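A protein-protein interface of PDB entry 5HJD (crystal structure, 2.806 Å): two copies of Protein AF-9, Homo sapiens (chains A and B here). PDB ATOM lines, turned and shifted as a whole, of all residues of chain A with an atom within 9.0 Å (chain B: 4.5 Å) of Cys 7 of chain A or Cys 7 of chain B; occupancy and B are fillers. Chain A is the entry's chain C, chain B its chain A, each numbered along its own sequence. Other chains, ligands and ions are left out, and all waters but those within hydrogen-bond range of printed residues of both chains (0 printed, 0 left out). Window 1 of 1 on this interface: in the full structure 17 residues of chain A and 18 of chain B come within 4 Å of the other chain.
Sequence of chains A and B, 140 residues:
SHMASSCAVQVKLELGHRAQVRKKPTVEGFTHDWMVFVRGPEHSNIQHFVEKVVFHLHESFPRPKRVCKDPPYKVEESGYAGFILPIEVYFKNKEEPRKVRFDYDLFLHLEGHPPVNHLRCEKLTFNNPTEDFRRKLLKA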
ATOM      1  N   ALA A   4      -2.576  19.659  -9.181  1.00  0.00           N
ATOM      2  CA  ALA A   4      -2.498  20.567 -10.326  1.00  0.00           C
ATOM      3  C   ALA A   4      -3.302  20.010 -11.506  1.00  0.00           C
ATOM      4  O   ALA A   4      -3.338  18.792 -11.664  1.00  0.00           O
ATOM      5  CB  ALA A   4      -1.044  20.779 -10.722  1.00  0.00           C
ATOM      6  N   SER A   5      -3.961  20.831 -12.336  1.00  0.00           N
ATOM      7  CA  SER A   5      -4.079  22.304 -12.298  1.00  0.00           C
ATOM      8  C   SER A   5      -2.764  23.090 -12.361  1.00  0.00           C
ATOM      9  O   SER A   5      -2.318  23.649 -11.361  1.00  0.00           O
ATOM     10  CB  SER A   5      -4.885  22.759 -11.071  1.00  0.00           C
ATOM     11  OG  SER A   5      -5.020  24.171 -11.044  1.00  0.00           O
ATOM     12  N   SER A   6      -2.162  23.134 -13.547  1.00  0.00           N
ATOM     13  CA  SER A   6      -1.005  23.985 -13.807  1.00  0.00           C
ATOM     14  C   SER A   6      -0.724  24.105 -15.299  1.00  0.00           C
ATOM     15  O   SER A   6      -0.284  23.153 -15.931  1.00  0.00           O
ATOM     16  CB  SER A   6       0.242  23.452 -13.103  1.00  0.00           C
ATOM     17  OG  SER A   6       1.388  24.210 -13.465  1.00  0.00           O
ATOM     18  N   CYS A   7      -0.977  25.276 -15.868  1.00  0.00           N
ATOM     19  CA  CYS A   7      -0.568  25.525 -17.245  1.00  0.00           C
ATOM     20  C   CYS A   7       0.531  26.574 -17.277  1.00  0.00           C
ATOM     21  O   CYS A   7       0.411  27.644 -16.686  1.00  0.00           O
ATOM     22  CB  CYS A   7      -1.743  25.967 -18.122  1.00  0.00           C
ATOM     23  SG  CYS A   7      -1.278  26.139 -19.871  1.00  0.00           S
ATOM     24  N   ALA A   8       1.617  26.234 -17.957  1.00  0.00           N
ATOM     25  CA  ALA A   8       2.743  27.142 -18.131  1.00  0.00           C
ATOM     26  C   ALA A   8       2.933  27.446 -19.607  1.00  0.00           C
ATOM     27  O   ALA A   8       3.386  26.600 -20.371  1.00  0.00           O
ATOM     28  CB  ALA A   8       4.008  26.545 -17.538  1.00  0.00           C
ATOM     29  N   VAL A   9       2.561  28.656 -20.007  1.00  0.00           N
ATOM     30  CA  VAL A   9       2.641  29.057 -21.404  1.00  0.00           C
ATOM     31  C   VAL A   9       3.910  29.852 -21.666  1.00  0.00           C
ATOM     32  O   VAL A   9       4.207  30.815 -20.963  1.00  0.00           O
ATOM     33  CB  VAL A   9       1.418  29.891 -21.819  1.00  0.00           C
ATOM     34  CG1 VAL A   9       1.506  30.265 -23.288  1.00  0.00           C
ATOM     35  CG2 VAL A   9       0.139  29.120 -21.541  1.00  0.00           C
ATOM     36  N   GLN A  10       4.662  29.440 -22.680  1.00  0.00           N
ATOM     37  CA  GLN A  10       5.925  30.089 -23.004  1.00  0.00           C
ATOM     38  C   GLN A  10       5.927  30.705 -24.398  1.00  0.00           C
ATOM     39  O   GLN A  10       5.586  30.048 -25.379  1.00  0.00           O
ATOM     40  CB  GLN A  10       7.078  29.090 -22.889  1.00  0.00           C
ATOM     41  CG  GLN A  10       7.327  28.579 -21.482  1.00  0.00           C
ATOM     42  CD  GLN A  10       8.509  27.632 -21.416  1.00  0.00           C
ATOM     43  OE1 GLN A  10       9.278  27.644 -20.453  1.00  0.00           O
ATOM     44  NE2 GLN A  10       8.660  26.803 -22.443  1.00  0.00           N
ATOM     45  N   VAL A  11       6.306  31.976 -24.476  1.00  0.00           N
ATOM     46  CA  VAL A  11       6.548  32.631 -25.756  1.00  0.00           C
ATOM     47  C   VAL A  11       7.975  33.167 -25.783  1.00  0.00           C
ATOM     48  O   VAL A  11       8.536  33.504 -24.741  1.00  0.00           O
ATOM     49  CB  VAL A  11       5.554  33.781 -26.019  1.00  0.00           C
ATOM     50  CG1 VAL A  11       4.161  33.229 -26.276  1.00  0.00           C
ATOM     51  CG2 VAL A  11       5.547  34.759 -24.855  1.00  0.00           C
ATOM     52  N   THR A 125       7.403  33.236 -19.555  1.00  0.00           N
ATOM     53  CA  THR A 125       6.543  32.158 -19.082  1.00  0.00           C
ATOM     54  C   THR A 125       5.365  32.700 -18.280  1.00  0.00           C
ATOM     55  O   THR A 125       5.550  33.348 -17.252  1.00  0.00           O
ATOM     56  CB  THR A 125       7.316  31.155 -18.206  1.00  0.00           C
ATOM     57  OG1 THR A 125       7.271  31.576 -16.837  1.00  0.00           O
ATOM     58  CG2 THR A 125       8.765  31.045 -18.658  1.00  0.00           C
ATOM     59  N   PHE A 126       4.153  32.425 -18.752  1.00  0.00           N
ATOM     60  CA  PHE A 126       2.947  32.829 -18.040  1.00  0.00           C
ATOM     61  C   PHE A 126       2.342  31.639 -17.303  1.00  0.00           C
ATOM     62  O   PHE A 126       1.967  30.644 -17.921  1.00  0.00           O
ATOM     63  CB  PHE A 126       1.919  33.426 -19.004  1.00  0.00           C
ATOM     64  CG  PHE A 126       2.381  34.686 -19.687  1.00  0.00           C
ATOM     65  CD1 PHE A 126       3.159  34.624 -20.832  1.00  0.00           C
ATOM     66  CD2 PHE A 126       2.029  35.930 -19.188  1.00  0.00           C
ATOM     67  CE1 PHE A 126       3.583  35.776 -21.463  1.00  0.00           C
ATOM     68  CE2 PHE A 126       2.450  37.088 -19.814  1.00  0.00           C
ATOM     69  CZ  PHE A 126       3.228  37.011 -20.954  1.00  0.00           C
ATOM     70  N   ASN A 127       2.247  31.747 -15.983  1.00  0.00           N
ATOM     71  CA  ASN A 127       1.682  30.675 -15.173  1.00  0.00           C
ATOM     72  C   ASN A 127       0.176  30.815 -15.000  1.00  0.00           C
ATOM     73  O   ASN A 127      -0.305  31.822 -14.481  1.00  0.00           O
ATOM     74  CB  ASN A 127       2.356  30.629 -13.802  1.00  0.00           C
ATOM     75  CG  ASN A 127       3.810  30.211 -13.884  1.00  0.00           C
ATOM     76  OD1 ASN A 127       4.148  29.220 -14.532  1.00  0.00           O
ATOM     77  ND2 ASN A 127       4.681  30.977 -13.239  1.00  0.00           N
ATOM     78  N   ASN A 128      -0.555  29.796 -15.441  1.00  0.00           N
ATOM     79  CA  ASN A 128      -2.012  29.772 -15.349  1.00  0.00           C
ATOM     80  C   ASN A 128      -2.688  31.004 -15.952  1.00  0.00           C
ATOM     81  O   ASN A 128      -3.331  31.768 -15.233  1.00  0.00           O
ATOM     82  CB  ASN A 128      -2.443  29.619 -13.886  1.00  0.00           C
ATOM     83  CG  ASN A 128      -2.036  28.284 -13.290  1.00  0.00           C
ATOM     84  OD1 ASN A 128      -2.371  27.223 -13.820  1.00  0.00           O
ATOM     85  ND2 ASN A 128      -1.306  28.331 -12.182  1.00  0.00           N
ATOM     86  N   PRO A 129      -2.546  31.208 -17.274  1.00  0.00           N
ATOM     87  CA  PRO A 129      -3.301  32.307 -17.883  1.00  0.00           C
ATOM     88  C   PRO A 129      -4.766  31.925 -18.014  1.00  0.00           C
ATOM     89  O   PRO A 129      -5.103  30.766 -17.785  1.00  0.00           O
ATOM     90  CB  PRO A 129      -2.648  32.460 -19.256  1.00  0.00           C
ATOM     91  CG  PRO A 129      -2.207  31.080 -19.587  1.00  0.00           C
ATOM     92  CD  PRO A 129      -1.739  30.486 -18.277  1.00  0.00           C
ATOM     93  N   THR A 130      -5.624  32.871 -18.380  1.00  0.00           N
ATOM     94  CA  THR A 130      -7.028  32.553 -18.610  1.00  0.00           C
ATOM     95  C   THR A 130      -7.170  31.732 -19.889  1.00  0.00           C
ATOM     96  O   THR A 130      -6.184  31.480 -20.583  1.00  0.00           O
ATOM     97  CB  THR A 130      -7.900  33.822 -18.716  1.00  0.00           C
ATOM     98  OG1 THR A 130      -7.493  34.594 -19.851  1.00  0.00           O
ATOM     99  CG2 THR A 130      -7.778  34.667 -17.451  1.00  0.00           C
ATOM    100  N   GLU A 131      -8.391  31.308 -20.199  1.00  0.00           N
ATOM    101  CA  GLU A 131      -8.642  30.631 -21.466  1.00  0.00           C
ATOM    102  C   GLU A 131      -8.454  31.629 -22.596  1.00  0.00           C
ATOM    103  O   GLU A 131      -7.804  31.340 -23.599  1.00  0.00           O
ATOM    104  CB  GLU A 131     -10.042  30.027 -21.509  1.00  0.00           C
ATOM    105  CG  GLU A 131     -10.040  28.537 -21.783  1.00  0.00           C
ATOM    106  CD  GLU A 131     -11.190  28.102 -22.663  1.00  0.00           C
ATOM    107  OE1 GLU A 131     -11.760  27.026 -22.400  1.00  0.00           O
ATOM    108  OE2 GLU A 131     -11.521  28.830 -23.621  1.00  0.00           O
ATOM    109  N   ARG A 134      -4.551  33.046 -23.602  1.00  0.00           N
ATOM    110  CA  ARG A 134      -3.784  31.852 -23.971  1.00  0.00           C
ATOM    111  C   ARG A 134      -4.030  31.486 -25.425  1.00  0.00           C
ATOM    112  O   ARG A 134      -3.127  31.043 -26.133  1.00  0.00           O
ATOM    113  CB  ARG A 134      -4.133  30.657 -23.078  1.00  0.00           C
ATOM    114  CG  ARG A 134      -3.257  29.435 -23.351  1.00  0.00           C
ATOM    115  CD  ARG A 134      -3.952  28.116 -23.057  1.00  0.00           C
ATOM    116  NE  ARG A 134      -4.051  27.254 -24.241  1.00  0.00           N
ATOM    117  CZ  ARG A 134      -4.026  25.921 -24.202  1.00  0.00           C
ATOM    118  NH1 ARG A 134      -4.110  25.226 -25.330  1.00  0.00           N
ATOM    119  NH2 ARG A 134      -3.918  25.275 -23.037  1.00  0.00           N
ATOM    120  N   LEU A 137      -1.642  33.611 -27.295  1.00  0.00           N
ATOM    121  CA  LEU A 137      -0.231  33.261 -27.135  1.00  0.00           C
ATOM    122  C   LEU A 137       0.198  32.081 -28.008  1.00  0.00           C
ATOM    123  O   LEU A 137       1.315  32.062 -28.526  1.00  0.00           O
ATOM    124  CB  LEU A 137       0.071  32.953 -25.665  1.00  0.00           C
ATOM    125  CG  LEU A 137       0.075  34.128 -24.679  1.00  0.00           C
ATOM    126  CD1 LEU A 137      -0.761  33.809 -23.453  1.00  0.00           C
ATOM    127  CD2 LEU A 137       1.492  34.483 -24.261  1.00  0.00           C
ATOM    128  N   LEU A 138      -0.687  31.101 -28.170  1.00  0.00           N
ATOM    129  CA  LEU A 138      -0.370  29.916 -28.962  1.00  0.00           C
ATOM    130  C   LEU A 138      -0.558  30.170 -30.455  1.00  0.00           C
ATOM    131  O   LEU A 138       0.054  29.502 -31.289  1.00  0.00           O
ATOM    132  CB  LEU A 138      -1.224  28.730 -28.516  1.00  0.00           C
ATOM    133  CG  LEU A 138      -0.899  28.190 -27.123  1.00  0.00           C
ATOM    134  CD1 LEU A 138      -1.762  26.986 -26.798  1.00  0.00           C
ATOM    135  CD2 LEU A 138       0.577  27.839 -27.012  1.00  0.00           C
ATOM    136  N   SER B   6       4.399  27.271 -26.507  1.00  0.00           N
ATOM    137  CA  SER B   6       4.056  25.955 -25.993  1.00  0.00           C
ATOM    138  C   SER B   6       3.546  25.969 -24.563  1.00  0.00           C
ATOM    139  O   SER B   6       4.116  26.623 -23.689  1.00  0.00           O
ATOM    140  CB  SER B   6       5.269  25.033 -26.088  1.00  0.00           C
ATOM    141  OG  SER B   6       6.377  25.607 -25.426  1.00  0.00           O
ATOM    142  N   CYS B   7       2.468  25.227 -24.337  1.00  0.00           N
ATOM    143  CA  CYS B   7       1.912  25.056 -23.002  1.00  0.00           C
ATOM    144  C   CYS B   7       2.244  23.676 -22.459  1.00  0.00           C
ATOM    145  O   CYS B   7       2.087  22.669 -23.148  1.00  0.00           O
ATOM    146  CB  CYS B   7       0.393  25.252 -23.003  1.00  0.00           C
ATOM    147  SG  CYS B   7      -0.388  25.121 -21.359  1.00  0.00           S
ATOM    148  N   ALA B   8       2.707  23.629 -21.217  1.00  0.00           N
ATOM    149  CA  ALA B   8       2.929  22.353 -20.554  1.00  0.00           C
ATOM    150  C   ALA B   8       2.002  22.227 -19.354  1.00  0.00           C
ATOM    151  O   ALA B   8       2.226  22.849 -18.317  1.00  0.00           O
ATOM    152  CB  ALA B   8       4.379  22.211 -20.132  1.00  0.00           C
ATOM    153  N   VAL B   9       0.957  21.421 -19.499  1.00  0.00           N
ATOM    154  CA  VAL B   9       0.012  21.211 -18.412  1.00  0.00           C
ATOM    155  C   VAL B   9       0.456  20.045 -17.537  1.00  0.00           C
ATOM    156  O   VAL B   9       0.635  18.923 -18.019  1.00  0.00           O
ATOM    157  CB  VAL B   9      -1.410  20.957 -18.939  1.00  0.00           C
ATOM    158  CG1 VAL B   9      -2.380  20.817 -17.781  1.00  0.00           C
ATOM    159  CG2 VAL B   9      -1.837  22.094 -19.850  1.00  0.00           C
ATOM    160  N   PHE B 126       1.536  17.108 -19.938  1.00  0.00           N
ATOM    161  CA  PHE B 126       0.892  17.144 -21.247  1.00  0.00           C
ATOM    162  C   PHE B 126       1.357  18.367 -22.030  1.00  0.00           C
ATOM    163  O   PHE B 126       1.242  19.495 -21.558  1.00  0.00           O
ATOM    164  CB  PHE B 126      -0.631  17.158 -21.100  1.00  0.00           C
ATOM    165  CG  PHE B 126      -1.190  15.926 -20.452  1.00  0.00           C
ATOM    166  CD1 PHE B 126      -1.546  14.828 -21.217  1.00  0.00           C
ATOM    167  CD2 PHE B 126      -1.368  15.867 -19.081  1.00  0.00           C
ATOM    168  CE1 PHE B 126      -2.064  13.692 -20.625  1.00  0.00           C
ATOM    169  CE2 PHE B 126      -1.885  14.734 -18.484  1.00  0.00           C
ATOM    170  CZ  PHE B 126      -2.233  13.645 -19.257  1.00  0.00           C
ATOM    171  N   ASN B 127       1.880  18.138 -23.230  1.00  0.00           N
ATOM    172  CA  ASN B 127       2.390  19.224 -24.058  1.00  0.00           C
ATOM    173  C   ASN B 127       1.404  19.640 -25.144  1.00  0.00           C
ATOM    174  O   ASN B 127       1.021  18.833 -25.991  1.00  0.00           O
ATOM    175  CB  ASN B 127       3.724  18.826 -24.695  1.00  0.00           C
ATOM    176  CG  ASN B 127       4.772  18.452 -23.665  1.00  0.00           C
ATOM    177  OD1 ASN B 127       5.340  19.317 -22.999  1.00  0.00           O
ATOM    178  ND2 ASN B 127       5.035  17.158 -23.532  1.00  0.00           N
ATOM    179  N   ASN B 128       1.006  20.907 -25.106  1.00  0.00           N
ATOM    180  CA  ASN B 128       0.075  21.481 -26.077  1.00  0.00           C
ATOM    181  C   ASN B 128      -1.192  20.656 -26.304  1.00  0.00           C
ATOM    182  O   ASN B 128      -1.442  20.204 -27.420  1.00  0.00           O
ATOM    183  CB  ASN B 128       0.781  21.688 -27.422  1.00  0.00           C
ATOM    184  CG  ASN B 128       2.034  22.530 -27.304  1.00  0.00           C
ATOM    185  OD1 ASN B 128       1.965  23.752 -27.188  1.00  0.00           O
ATOM    186  ND2 ASN B 128       3.193  21.878 -27.348  1.00  0.00           N
ATOM    187  N   PRO B 129      -1.998  20.452 -25.248  1.00  0.00           N
ATOM    188  CA  PRO B 129      -3.244  19.707 -25.450  1.00  0.00           C
ATOM    189  C   PRO B 129      -4.332  20.592 -26.041  1.00  0.00           C
ATOM    190  O   PRO B 129      -4.180  21.813 -26.041  1.00  0.00           O
ATOM    191  CB  PRO B 129      -3.611  19.270 -24.036  1.00  0.00           C
ATOM    192  CG  PRO B 129      -3.126  20.399 -23.193  1.00  0.00           C
ATOM    193  CD  PRO B 129      -1.838  20.863 -23.839  1.00  0.00           C
ATOM    194  N   ARG B 134      -7.829  20.357 -21.961  1.00  0.00           N
ATOM    195  CA  ARG B 134      -7.008  21.125 -21.030  1.00  0.00           C
ATOM    196  C   ARG B 134      -7.790  21.622 -19.811  1.00  0.00           C
ATOM    197  O   ARG B 134      -7.259  21.659 -18.702  1.00  0.00           O
ATOM    198  CB  ARG B 134      -6.369  22.302 -21.767  1.00  0.00           C
ATOM    199  CG  ARG B 134      -5.504  23.219 -20.925  1.00  0.00           C
ATOM    200  CD  ARG B 134      -6.150  24.595 -20.854  1.00  0.00           C
ATOM    201  NE  ARG B 134      -5.263  25.624 -20.338  1.00  0.00           N
ATOM    202  CZ  ARG B 134      -5.646  26.877 -20.113  1.00  0.00           C
ATOM    203  NH1 ARG B 134      -6.900  27.243 -20.358  1.00  0.00           N
ATOM    204  NH2 ARG B 134      -4.787  27.770 -19.637  1.00  0.00           N
ATOM    205  N   LEU B 138      -7.292  21.065 -15.668  1.00  0.00           N
ATOM    206  CA  LEU B 138      -7.221  22.180 -14.731  1.00  0.00           C
ATOM    207  C   LEU B 138      -8.371  22.166 -13.725  1.00  0.00           C
ATOM    208  O   LEU B 138      -8.314  22.848 -12.703  1.00  0.00           O
ATOM    209  CB  LEU B 138      -7.207  23.512 -15.487  1.00  0.00           C
ATOM    210  CG  LEU B 138      -6.002  23.787 -16.392  1.00  0.00           C
ATOM    211  CD1 LEU B 138      -6.142  25.138 -17.078  1.00  0.00           C
ATOM    212  CD2 LEU B 138      -4.702  23.720 -15.608  1.00  0.00           C
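Cys 7 of chain B touches its own counterpart, Cys 7 of chain A.
Ala 8 of chain A touches Cys 7 of chain B, but with the chains exchanged Cys 7 of chain A does not touch Ala 8 of chain B (4.01 Å).
Ala 8 of chain B touches its own counterpart, Ala 8 of chain A.
Pro 129 of chain A touches Arg 134 of chain B, and with the chains exchanged Arg 134 of chain A touches Pro 129 of chain B.
10 positions are printed for both chains.
Of the 17 pairs that touch across the chains among the printed residues, 13 have their exchanged pair printed and touching as well.
Of the printed residues of chain B, Cys 7 of chain A touches Cys 7 and Arg 134.
Cys 7 of chain B touches just these residues of chain A: Cys 7, Ala 8 and Arg 134.
Of the printed residues of chain A, Val 9 of chain B touches Ser 6.
Of the printed residues of chain B, Val 9 of chain A touches Ser 6 (3.6 Å).
Printed residues of chain B within 4 Å of Leu 138 of chain A: Ser 6.
Of the printed residues of chain B, Ser 5 of chain A touches Leu 138.
Ala 4 of chain A touches none of the printed residues of chain B.
The nearest printed residue of chain B that does not touch Leu 138 of chain A is Cys 7 of chain B (4.2 Å).
Of the 18 printed residues of chain A, 10 touch a printed residue of chain B.
Printed residues of chain A that touch a printed residue of chain B: Ser 5, Ser 6, Cys 7, Ala 8, Val 9, Gln 10, Pro 129, Glu 131, Arg 134 and Leu 138.
Among the printed residues, 17 pairs touch across the chains.
The backbone carbonyl oxygen (O) of Cys 7 of chain B sits at hydrogen-bond distance from the backbone NH (N) of Asn 128 of chain B, 2.8 Å away.
N of Phe 126 of chain B lies within hydrogen-bond range of O of Val 9 of chain B (2.8 Å).
The backbone carbonyl oxygen (O) of Cys 7 of chain A lies within hydrogen-bond range of the backbone NH (N) of Asn 128 of chain A.
N of Phe 126 of chain A is in hydrogen-bond range of O of Val 9 of chain A.
Among the printed residues, merely in contact across the chains: Ser 6 of chain A with Val 9 of chain B (3.2 Å), Ser 6 of chain A with Leu 138 of chain B (3.3 Å), Ala 8 of chain A with Cys 7 of chain B (3.4 Å), Pro 129 of chain A with Arg 134 of chain B (3.5 Å), Val 9 of chain A with Ser 6 of chain B (3.6 Å), Ser 5 of chain A with Leu 138 of chain B (3.7 Å), Glu 131 of chain A with Arg 134 of chain B (3.7 Å), Cys 7 of chain A with Arg 134 of chain B (3.8 Å), Leu 138 of chain A with Ser 6 of chain B (3.9 Å) and Arg 134 of chain A with Cys 7 of chain B (3.9 Å).
O of Ser 6 of chain B sits at hydrogen-bond distance from N of Gln 10 of chain A.
The side-chain sulfur (SG) of Cys 7 of chain B is disulfide-bonded to the side-chain sulfur (SG) of Cys 7 of chain A, 2.0 Å away.
The backbone NH of Ala 8 of chain B lies within hydrogen-bond range of the backbone carbonyl oxygen of Ala 8 of chain A (3.2 Å).
O of Pro 129 of chain B sits at hydrogen-bond distance from NH1 of Arg 134 of chain A (3.5 Å).
The backbone carbonyl oxygen (O) of Ser 6 of chain A lies close to the backbone carbonyl oxygen (O) of Ala 8 of chain B.
The backbone carbonyl oxygen of Ser 6 of chain B lies close to the backbone carbonyl oxygen of Ala 8 of chain A.
The guanidinium group of Arg 134 of chain B sits close to the guanidinium group of Arg 134 of chain A.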
